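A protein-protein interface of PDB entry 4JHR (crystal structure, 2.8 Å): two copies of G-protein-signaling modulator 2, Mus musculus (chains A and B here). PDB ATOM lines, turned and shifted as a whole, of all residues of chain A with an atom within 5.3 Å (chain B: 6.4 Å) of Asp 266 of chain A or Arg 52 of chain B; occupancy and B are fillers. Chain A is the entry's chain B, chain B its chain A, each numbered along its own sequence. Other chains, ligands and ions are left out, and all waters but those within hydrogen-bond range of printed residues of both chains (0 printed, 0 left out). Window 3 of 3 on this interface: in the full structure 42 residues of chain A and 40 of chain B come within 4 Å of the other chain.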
ATOM      1  N   ARG A 262      16.983   8.943 -10.710  1.00  0.00           N
ATOM      2  CA  ARG A 262      17.091   9.559 -12.034  1.00  0.00           C
ATOM      3  C   ARG A 262      16.364   8.782 -13.143  1.00  0.00           C
ATOM      4  O   ARG A 262      15.656   9.384 -13.964  1.00  0.00           O
ATOM      5  CB  ARG A 262      18.575   9.787 -12.412  1.00  0.00           C
ATOM      6  N   GLU A 263      16.523   7.455 -13.146  1.00  0.00           N
ATOM      7  CA  GLU A 263      15.991   6.614 -14.223  1.00  0.00           C
ATOM      8  C   GLU A 263      14.484   6.299 -14.120  1.00  0.00           C
ATOM      9  O   GLU A 263      13.808   6.121 -15.136  1.00  0.00           O
ATOM     10  CB  GLU A 263      16.802   5.324 -14.348  1.00  0.00           C
ATOM     11  CG  GLU A 263      16.261   4.168 -13.543  1.00  0.00           C
ATOM     12  CD  GLU A 263      17.268   3.033 -13.402  1.00  0.00           C
ATOM     13  OE1 GLU A 263      16.833   1.863 -13.250  1.00  0.00           O
ATOM     14  OE2 GLU A 263      18.493   3.313 -13.435  1.00  0.00           O
ATOM     15  N   VAL A 264      13.951   6.242 -12.908  1.00  0.00           N
ATOM     16  CA  VAL A 264      12.528   5.981 -12.752  1.00  0.00           C
ATOM     17  C   VAL A 264      11.663   7.209 -13.037  1.00  0.00           C
ATOM     18  O   VAL A 264      10.447   7.091 -13.148  1.00  0.00           O
ATOM     19  CB  VAL A 264      12.189   5.428 -11.358  1.00  0.00           C
ATOM     20  CG1 VAL A 264      13.222   4.368 -10.939  1.00  0.00           C
ATOM     21  CG2 VAL A 264      12.104   6.564 -10.339  1.00  0.00           C
ATOM     22  N   GLY A 265      12.279   8.383 -13.158  1.00  0.00           N
ATOM     23  CA  GLY A 265      11.551   9.574 -13.566  1.00  0.00           C
ATOM     24  C   GLY A 265      11.265   9.588 -15.061  1.00  0.00           C
ATOM     25  O   GLY A 265      10.202  10.053 -15.506  1.00  0.00           O
ATOM     26  N   ASP A 266      12.213   9.062 -15.838  1.00  0.00           N
ATOM     27  CA  ASP A 266      12.086   9.008 -17.296  1.00  0.00           C
ATOM     28  C   ASP A 266      11.113   7.915 -17.744  1.00  0.00           C
ATOM     29  O   ASP A 266      10.767   7.830 -18.924  1.00  0.00           O
ATOM     30  CB  ASP A 266      13.455   8.786 -17.963  1.00  0.00           C
ATOM     31  CG  ASP A 266      14.397   9.986 -17.817  1.00  0.00           C
ATOM     32  OD1 ASP A 266      15.606   9.807 -18.074  1.00  0.00           O
ATOM     33  OD2 ASP A 266      13.940  11.094 -17.449  1.00  0.00           O
ATOM     34  N   LEU A 267      10.683   7.091 -16.789  1.00  0.00           N
ATOM     35  CA  LEU A 267       9.804   5.950 -17.032  1.00  0.00           C
ATOM     36  C   LEU A 267       8.368   6.368 -17.333  1.00  0.00           C
ATOM     37  O   LEU A 267       7.898   7.397 -16.837  1.00  0.00           O
ATOM     38  CB  LEU A 267       9.835   5.053 -15.808  1.00  0.00           C
ATOM     39  CG  LEU A 267      10.399   3.630 -15.932  1.00  0.00           C
ATOM     40  CD1 LEU A 267      11.358   3.373 -17.088  1.00  0.00           C
ATOM     41  CD2 LEU A 267      10.889   3.025 -14.620  1.00  0.00           C
ATOM     42  N   GLU A 268       7.677   5.558 -18.137  1.00  0.00           N
ATOM     43  CA  GLU A 268       6.312   5.863 -18.572  1.00  0.00           C
ATOM     44  C   GLU A 268       5.305   4.759 -18.250  1.00  0.00           C
ATOM     45  O   GLU A 268       4.093   4.995 -18.250  1.00  0.00           O
ATOM     46  CB  GLU A 268       6.286   6.159 -20.069  1.00  0.00           C
ATOM     47  CG  GLU A 268       7.346   7.139 -20.508  1.00  0.00           C
ATOM     48  CD  GLU A 268       7.094   7.693 -21.904  1.00  0.00           C
ATOM     49  OE1 GLU A 268       5.912   7.948 -22.248  1.00  0.00           O
ATOM     50  OE2 GLU A 268       8.086   7.879 -22.656  1.00  0.00           O
ATOM     51  N   GLN A 294      15.027  16.305  -7.746  1.00  0.00           N
ATOM     52  CA  GLN A 294      13.644  15.880  -7.539  1.00  0.00           C
ATOM     53  C   GLN A 294      13.193  15.080  -8.750  1.00  0.00           C
ATOM     54  O   GLN A 294      13.452  15.473  -9.888  1.00  0.00           O
ATOM     55  CB  GLN A 294      12.729  17.087  -7.409  1.00  0.00           C
ATOM     56  CG  GLN A 294      12.879  17.875  -6.140  1.00  0.00           C
ATOM     57  CD  GLN A 294      11.715  18.817  -5.962  1.00  0.00           C
ATOM     58  OE1 GLN A 294      10.880  18.968  -6.869  1.00  0.00           O
ATOM     59  NE2 GLN A 294      11.639  19.452  -4.791  1.00  0.00           N
ATOM     60  N   ARG A 295      12.516  13.963  -8.509  1.00  0.00           N
ATOM     61  CA  ARG A 295      12.026  13.117  -9.581  1.00  0.00           C
ATOM     62  C   ARG A 295      10.627  12.683  -9.233  1.00  0.00           C
ATOM     63  O   ARG A 295      10.311  12.431  -8.060  1.00  0.00           O
ATOM     64  CB  ARG A 295      12.884  11.849  -9.757  1.00  0.00           C
ATOM     65  CG  ARG A 295      14.162  12.002 -10.548  1.00  0.00           C
ATOM     66  CD  ARG A 295      13.939  12.773 -11.826  1.00  0.00           C
ATOM     67  NE  ARG A 295      14.466  14.129 -11.702  1.00  0.00           N
ATOM     68  CZ  ARG A 295      15.648  14.525 -12.170  1.00  0.00           C
ATOM     69  NH1 ARG A 295      16.437  13.671 -12.821  1.00  0.00           N
ATOM     70  NH2 ARG A 295      16.035  15.784 -11.987  1.00  0.00           N
ATOM     71  N   CYS A 296       9.799  12.564 -10.264  1.00  0.00           N
ATOM     72  CA  CYS A 296       8.450  12.061 -10.098  1.00  0.00           C
ATOM     73  C   CYS A 296       7.977  11.446 -11.406  1.00  0.00           C
ATOM     74  O   CYS A 296       8.133  12.047 -12.474  1.00  0.00           O
ATOM     75  CB  CYS A 296       7.513  13.190  -9.690  1.00  0.00           C
ATOM     76  SG  CYS A 296       5.884  12.634  -9.188  1.00  0.00           S
ATOM     77  N   HIS B  37      11.405  24.128  -6.552  1.00  0.00           N
ATOM     78  CA  HIS B  37      12.335  23.718  -7.595  1.00  0.00           C
ATOM     79  C   HIS B  37      12.203  24.576  -8.850  1.00  0.00           C
ATOM     80  O   HIS B  37      13.185  25.072  -9.382  1.00  0.00           O
ATOM     81  CB  HIS B  37      12.069  22.253  -7.938  1.00  0.00           C
ATOM     82  CG  HIS B  37      12.955  21.709  -9.011  1.00  0.00           C
ATOM     83  ND1 HIS B  37      14.087  22.359  -9.447  1.00  0.00           N
ATOM     84  CD2 HIS B  37      12.880  20.567  -9.735  1.00  0.00           C
ATOM     85  CE1 HIS B  37      14.666  21.652 -10.400  1.00  0.00           C
ATOM     86  NE2 HIS B  37      13.957  20.556 -10.590  1.00  0.00           N
ATOM     87  N   LYS B  47      17.087  26.207 -17.884  1.00  0.00           N
ATOM     88  CA  LYS B  47      16.094  25.714 -18.836  1.00  0.00           C
ATOM     89  C   LYS B  47      15.755  24.229 -18.643  1.00  0.00           C
ATOM     90  O   LYS B  47      14.591  23.839 -18.740  1.00  0.00           O
ATOM     91  CB  LYS B  47      16.586  25.966 -20.265  1.00  0.00           C
ATOM     92  CG  LYS B  47      15.614  26.693 -21.177  1.00  0.00           C
ATOM     93  CD  LYS B  47      15.293  28.087 -20.680  1.00  0.00           C
ATOM     94  CE  LYS B  47      13.885  28.150 -20.109  1.00  0.00           C
ATOM     95  NZ  LYS B  47      13.388  29.539 -19.974  1.00  0.00           N
ATOM     96  N   VAL B  48      16.768  23.410 -18.367  1.00  0.00           N
ATOM     97  CA  VAL B  48      16.554  21.980 -18.148  1.00  0.00           C
ATOM     98  C   VAL B  48      15.730  21.741 -16.909  1.00  0.00           C
ATOM     99  O   VAL B  48      14.668  21.117 -16.968  1.00  0.00           O
ATOM    100  CB  VAL B  48      17.891  21.199 -17.995  1.00  0.00           C
ATOM    101  CG1 VAL B  48      17.657  19.848 -17.314  1.00  0.00           C
ATOM    102  CG2 VAL B  48      18.584  21.019 -19.356  1.00  0.00           C
ATOM    103  N   GLY B  49      16.227  22.234 -15.782  1.00  0.00           N
ATOM    104  CA  GLY B  49      15.562  22.027 -14.510  1.00  0.00           C
ATOM    105  C   GLY B  49      14.165  22.615 -14.433  1.00  0.00           C
ATOM    106  O   GLY B  49      13.313  22.084 -13.724  1.00  0.00           O
ATOM    107  N   GLU B  50      13.926  23.712 -15.145  1.00  0.00           N
ATOM    108  CA  GLU B  50      12.589  24.284 -15.192  1.00  0.00           C
ATOM    109  C   GLU B  50      11.663  23.264 -15.836  1.00  0.00           C
ATOM    110  O   GLU B  50      10.564  23.005 -15.341  1.00  0.00           O
ATOM    111  CB  GLU B  50      12.577  25.589 -15.999  1.00  0.00           C
ATOM    112  CG  GLU B  50      11.366  26.463 -15.739  1.00  0.00           C
ATOM    113  CD  GLU B  50      11.091  27.464 -16.849  1.00  0.00           C
ATOM    114  OE1 GLU B  50      10.110  28.246 -16.751  1.00  0.00           O
ATOM    115  OE2 GLU B  50      11.858  27.461 -17.828  1.00  0.00           O
ATOM    116  N   ALA B  51      12.127  22.675 -16.937  1.00  0.00           N
ATOM    117  CA  ALA B  51      11.331  21.695 -17.670  1.00  0.00           C
ATOM    118  C   ALA B  51      11.064  20.480 -16.802  1.00  0.00           C
ATOM    119  O   ALA B  51      10.021  19.843 -16.896  1.00  0.00           O
ATOM    120  CB  ALA B  51      12.037  21.285 -18.972  1.00  0.00           C
ATOM    121  N   ARG B  52      12.024  20.155 -15.957  1.00  0.00           N
ATOM    122  CA  ARG B  52      11.870  18.968 -15.145  1.00  0.00           C
ATOM    123  C   ARG B  52      10.858  19.269 -14.069  1.00  0.00           C
ATOM    124  O   ARG B  52       9.982  18.451 -13.798  1.00  0.00           O
ATOM    125  CB  ARG B  52      13.203  18.514 -14.546  1.00  0.00           C
ATOM    126  CG  ARG B  52      13.078  17.342 -13.613  1.00  0.00           C
ATOM    127  CD  ARG B  52      12.436  16.168 -14.303  1.00  0.00           C
ATOM    128  NE  ARG B  52      13.342  15.513 -15.245  1.00  0.00           N
ATOM    129  CZ  ARG B  52      13.245  14.235 -15.619  1.00  0.00           C
ATOM    130  NH1 ARG B  52      12.284  13.455 -15.129  1.00  0.00           N
ATOM    131  NH2 ARG B  52      14.111  13.734 -16.485  1.00  0.00           N
ATOM    132  N   ALA B  53      10.966  20.445 -13.460  1.00  0.00           N
ATOM    133  CA  ALA B  53      10.032  20.822 -12.402  1.00  0.00           C
ATOM    134  C   ALA B  53       8.605  20.879 -12.940  1.00  0.00           C
ATOM    135  O   ALA B  53       7.653  20.573 -12.221  1.00  0.00           O
ATOM    136  CB  ALA B  53      10.414  22.146 -11.803  1.00  0.00           C
ATOM    137  N   LEU B  54       8.473  21.269 -14.206  1.00  0.00           N
ATOM    138  CA  LEU B  54       7.171  21.353 -14.841  1.00  0.00           C
ATOM    139  C   LEU B  54       6.548  19.967 -15.027  1.00  0.00           C
ATOM    140  O   LEU B  54       5.356  19.774 -14.776  1.00  0.00           O
ATOM    141  CB  LEU B  54       7.263  22.129 -16.169  1.00  0.00           C
ATOM    142  CG  LEU B  54       7.390  23.661 -16.050  1.00  0.00           C
ATOM    143  CD1 LEU B  54       7.180  24.316 -17.362  1.00  0.00           C
ATOM    144  CD2 LEU B  54       6.404  24.236 -15.064  1.00  0.00           C
ATOM    145  N   TYR B  55       7.373  19.021 -15.463  1.00  0.00           N
ATOM    146  CA  TYR B  55       7.013  17.612 -15.567  1.00  0.00           C
ATOM    147  C   TYR B  55       6.626  17.030 -14.218  1.00  0.00           C
ATOM    148  O   TYR B  55       5.597  16.376 -14.082  1.00  0.00           O
ATOM    149  CB  TYR B  55       8.207  16.836 -16.126  1.00  0.00           C
ATOM    150  CG  TYR B  55       7.929  15.395 -16.530  1.00  0.00           C
ATOM    151  CD1 TYR B  55       7.125  15.089 -17.632  1.00  0.00           C
ATOM    152  CD2 TYR B  55       8.510  14.343 -15.838  1.00  0.00           C
ATOM    153  CE1 TYR B  55       6.889  13.754 -18.013  1.00  0.00           C
ATOM    154  CE2 TYR B  55       8.283  13.015 -16.206  1.00  0.00           C
ATOM    155  CZ  TYR B  55       7.470  12.724 -17.292  1.00  0.00           C
ATOM    156  OH  TYR B  55       7.250  11.404 -17.650  1.00  0.00           O
ATOM    157  N   ASN B  56       7.461  17.261 -13.211  1.00  0.00           N
ATOM    158  CA  ASN B  56       7.174  16.736 -11.885  1.00  0.00           C
ATOM    159  C   ASN B  56       5.839  17.250 -11.365  1.00  0.00           C
ATOM    160  O   ASN B  56       5.013  16.484 -10.871  1.00  0.00           O
ATOM    161  CB  ASN B  56       8.300  17.088 -10.933  1.00  0.00           C
ATOM    162  CG  ASN B  56       9.578  16.376 -11.279  1.00  0.00           C
ATOM    163  OD1 ASN B  56       9.559  15.256 -11.809  1.00  0.00           O
ATOM    164  ND2 ASN B  56      10.708  17.015 -10.976  1.00  0.00           N
ATOM    165  N   LEU B  57       5.641  18.557 -11.516  1.00  0.00           N
ATOM    166  CA  LEU B  57       4.439  19.245 -11.083  1.00  0.00           C
ATOM    167  C   LEU B  57       3.208  18.806 -11.896  1.00  0.00           C
ATOM    168  O   LEU B  57       2.114  18.681 -11.352  1.00  0.00           O
ATOM    169  CB  LEU B  57       4.659  20.747 -11.213  1.00  0.00           C
ATOM    170  CG  LEU B  57       3.820  21.680 -10.351  1.00  0.00           C
ATOM    171  CD1 LEU B  57       3.819  21.246  -8.887  1.00  0.00           C
ATOM    172  CD2 LEU B  57       4.391  23.068 -10.505  1.00  0.00           C
ATOM    173  N   ASN B  97       5.864  22.431 -20.366  1.00  0.00           N
ATOM    174  CA  ASN B  97       7.027  21.566 -20.459  1.00  0.00           C
ATOM    175  C   ASN B  97       7.340  21.132 -21.890  1.00  0.00           C
ATOM    176  O   ASN B  97       8.491  21.195 -22.323  1.00  0.00           O
ATOM    177  CB  ASN B  97       6.841  20.327 -19.592  1.00  0.00           C
ATOM    178  CG  ASN B  97       7.822  19.217 -19.948  1.00  0.00           C
ATOM    179  OD1 ASN B  97       7.502  18.338 -20.738  1.00  0.00           O
ATOM    180  ND2 ASN B  97       9.028  19.266 -19.374  1.00  0.00           N
ATOM    181  N   LEU B 100       9.078  23.529 -24.138  1.00  0.00           N
ATOM    182  CA  LEU B 100      10.399  23.767 -23.582  1.00  0.00           C
ATOM    183  C   LEU B 100      11.368  22.666 -23.990  1.00  0.00           C
ATOM    184  O   LEU B 100      12.461  22.920 -24.491  1.00  0.00           O
ATOM    185  CB  LEU B 100      10.278  23.784 -22.055  1.00  0.00           C
ATOM    186  CG  LEU B 100      11.200  24.670 -21.249  1.00  0.00           C
ATOM    187  CD1 LEU B 100      11.074  26.082 -21.756  1.00  0.00           C
ATOM    188  CD2 LEU B 100      10.817  24.597 -19.809  1.00  0.00           C
ATOM    189  N   ARG B 112       7.502  11.907 -23.594  1.00  0.00           N
ATOM    190  CA  ARG B 112       6.959  11.670 -22.268  1.00  0.00           C
ATOM    191  C   ARG B 112       5.796  12.613 -22.007  1.00  0.00           C
ATOM    192  O   ARG B 112       4.753  12.203 -21.471  1.00  0.00           O
ATOM    193  CB  ARG B 112       8.042  11.823 -21.197  1.00  0.00           C
ATOM    194  CG  ARG B 112       9.190  10.829 -21.345  1.00  0.00           C
ATOM    195  CD  ARG B 112      10.027  10.702 -20.085  1.00  0.00           C
ATOM    196  NE  ARG B 112      10.728  11.940 -19.760  1.00  0.00           N
ATOM    197  CZ  ARG B 112      11.941  12.249 -20.208  1.00  0.00           C
ATOM    198  NH1 ARG B 112      12.581  11.398 -21.005  1.00  0.00           N
ATOM    199  NH2 ARG B 112      12.510  13.402 -19.856  1.00  0.00           N
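The backbone NH (N) of Cys 296 of chain A is in hydrogen-bond range of the side-chain amide oxygen (OD1) of Asn 56 of chain B (3.1 Å). The guanidinium group (NH2) of Arg 52 of chain B is in salt-bridge range of the side-chain carboxylate (OD2) of Asp 266 of chain A. The side-chain amide nitrogen (ND2) of Asn 56 of chain B is in hydrogen-bond range of the backbone carbonyl oxygen (O) of Gln 294 of chain A, 3.3 Å away. The guanidinium group (NH2) of Arg 112 of chain B is in salt-bridge range of the side-chain carboxylate (OD2) of Asp 266 of chain A, 3.6 Å away.
The backbone carbonyl oxygen of Arg 52 of chain B is in hydrogen-bond range of the side-chain amide nitrogen of Asn 56 of chain B (3.2 Å).
Arg 52 of chain B touches Gly 265 of chain A (NH1 to C, 3.9996 Å). O of Gly 265 of chain A touches CE2 of Tyr 55 of chain B, 3.6 Å away. Glu 268 of chain A touches Arg 112 of chain B. Gln 294 of chain A touches His 37 of chain B. Arg 52 of chain B touches Arg 295 of chain A (CG to NH2, 3.7 Å). C of Arg 295 of chain A touches OD1 of Asn 56 of chain B (3.8 Å). Cys 296 of chain A touches Tyr 55 of chain B (O to CE2, 3.9 Å).
Glu 263 of chain A touches none of the printed residues of chain B. Asp 266 of chain A touches just these residues of chain B: Arg 52 and Arg 112. Leu 267 of chain A touches none of the printed residues of chain B. Printed residues of chain B within 4 Å of Gln 294 of chain A: His 37 (3.7 Å) and Asn 56 (3.3 Å). Of the printed residues of chain B, Arg 295 of chain A touches Arg 52 and Asn 56. Of the printed residues of chain A, Arg 52 of chain B touches Gly 265, Asp 266 and Arg 295. Of the printed residues of chain A, Tyr 55 of chain B touches Gly 265 and Cys 296. Of the printed residues of chain A, Asn 56 of chain B touches Gln 294, Arg 295 and Cys 296. Of the printed residues of chain A, Arg 112 of chain B touches Asp 266 and Glu 268. The nearest printed residue of chain A that does not touch Arg 52 of chain B is Gln 294 of chain A (4.2 Å).
Printed residues of chain A that touch a printed residue of chain B: Gly 265, Asp 266, Glu 268, Gln 294, Arg 295 and Cys 296. Of the 15 printed residues of chain B, 5 touch a printed residue of chain A. Among the printed residues, Asp or Glu carboxylates within 4 Å of a Lys or Arg side-chain nitrogen of the other chain: Asp 266 of chain A with Arg 52 of chain B and Asp 266 of chain A with Arg 112 of chain B.
No position is printed for both chains. Of the 11 pairs that touch across the chains among the printed residues, none has its exchanged pair printed and touching as well.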
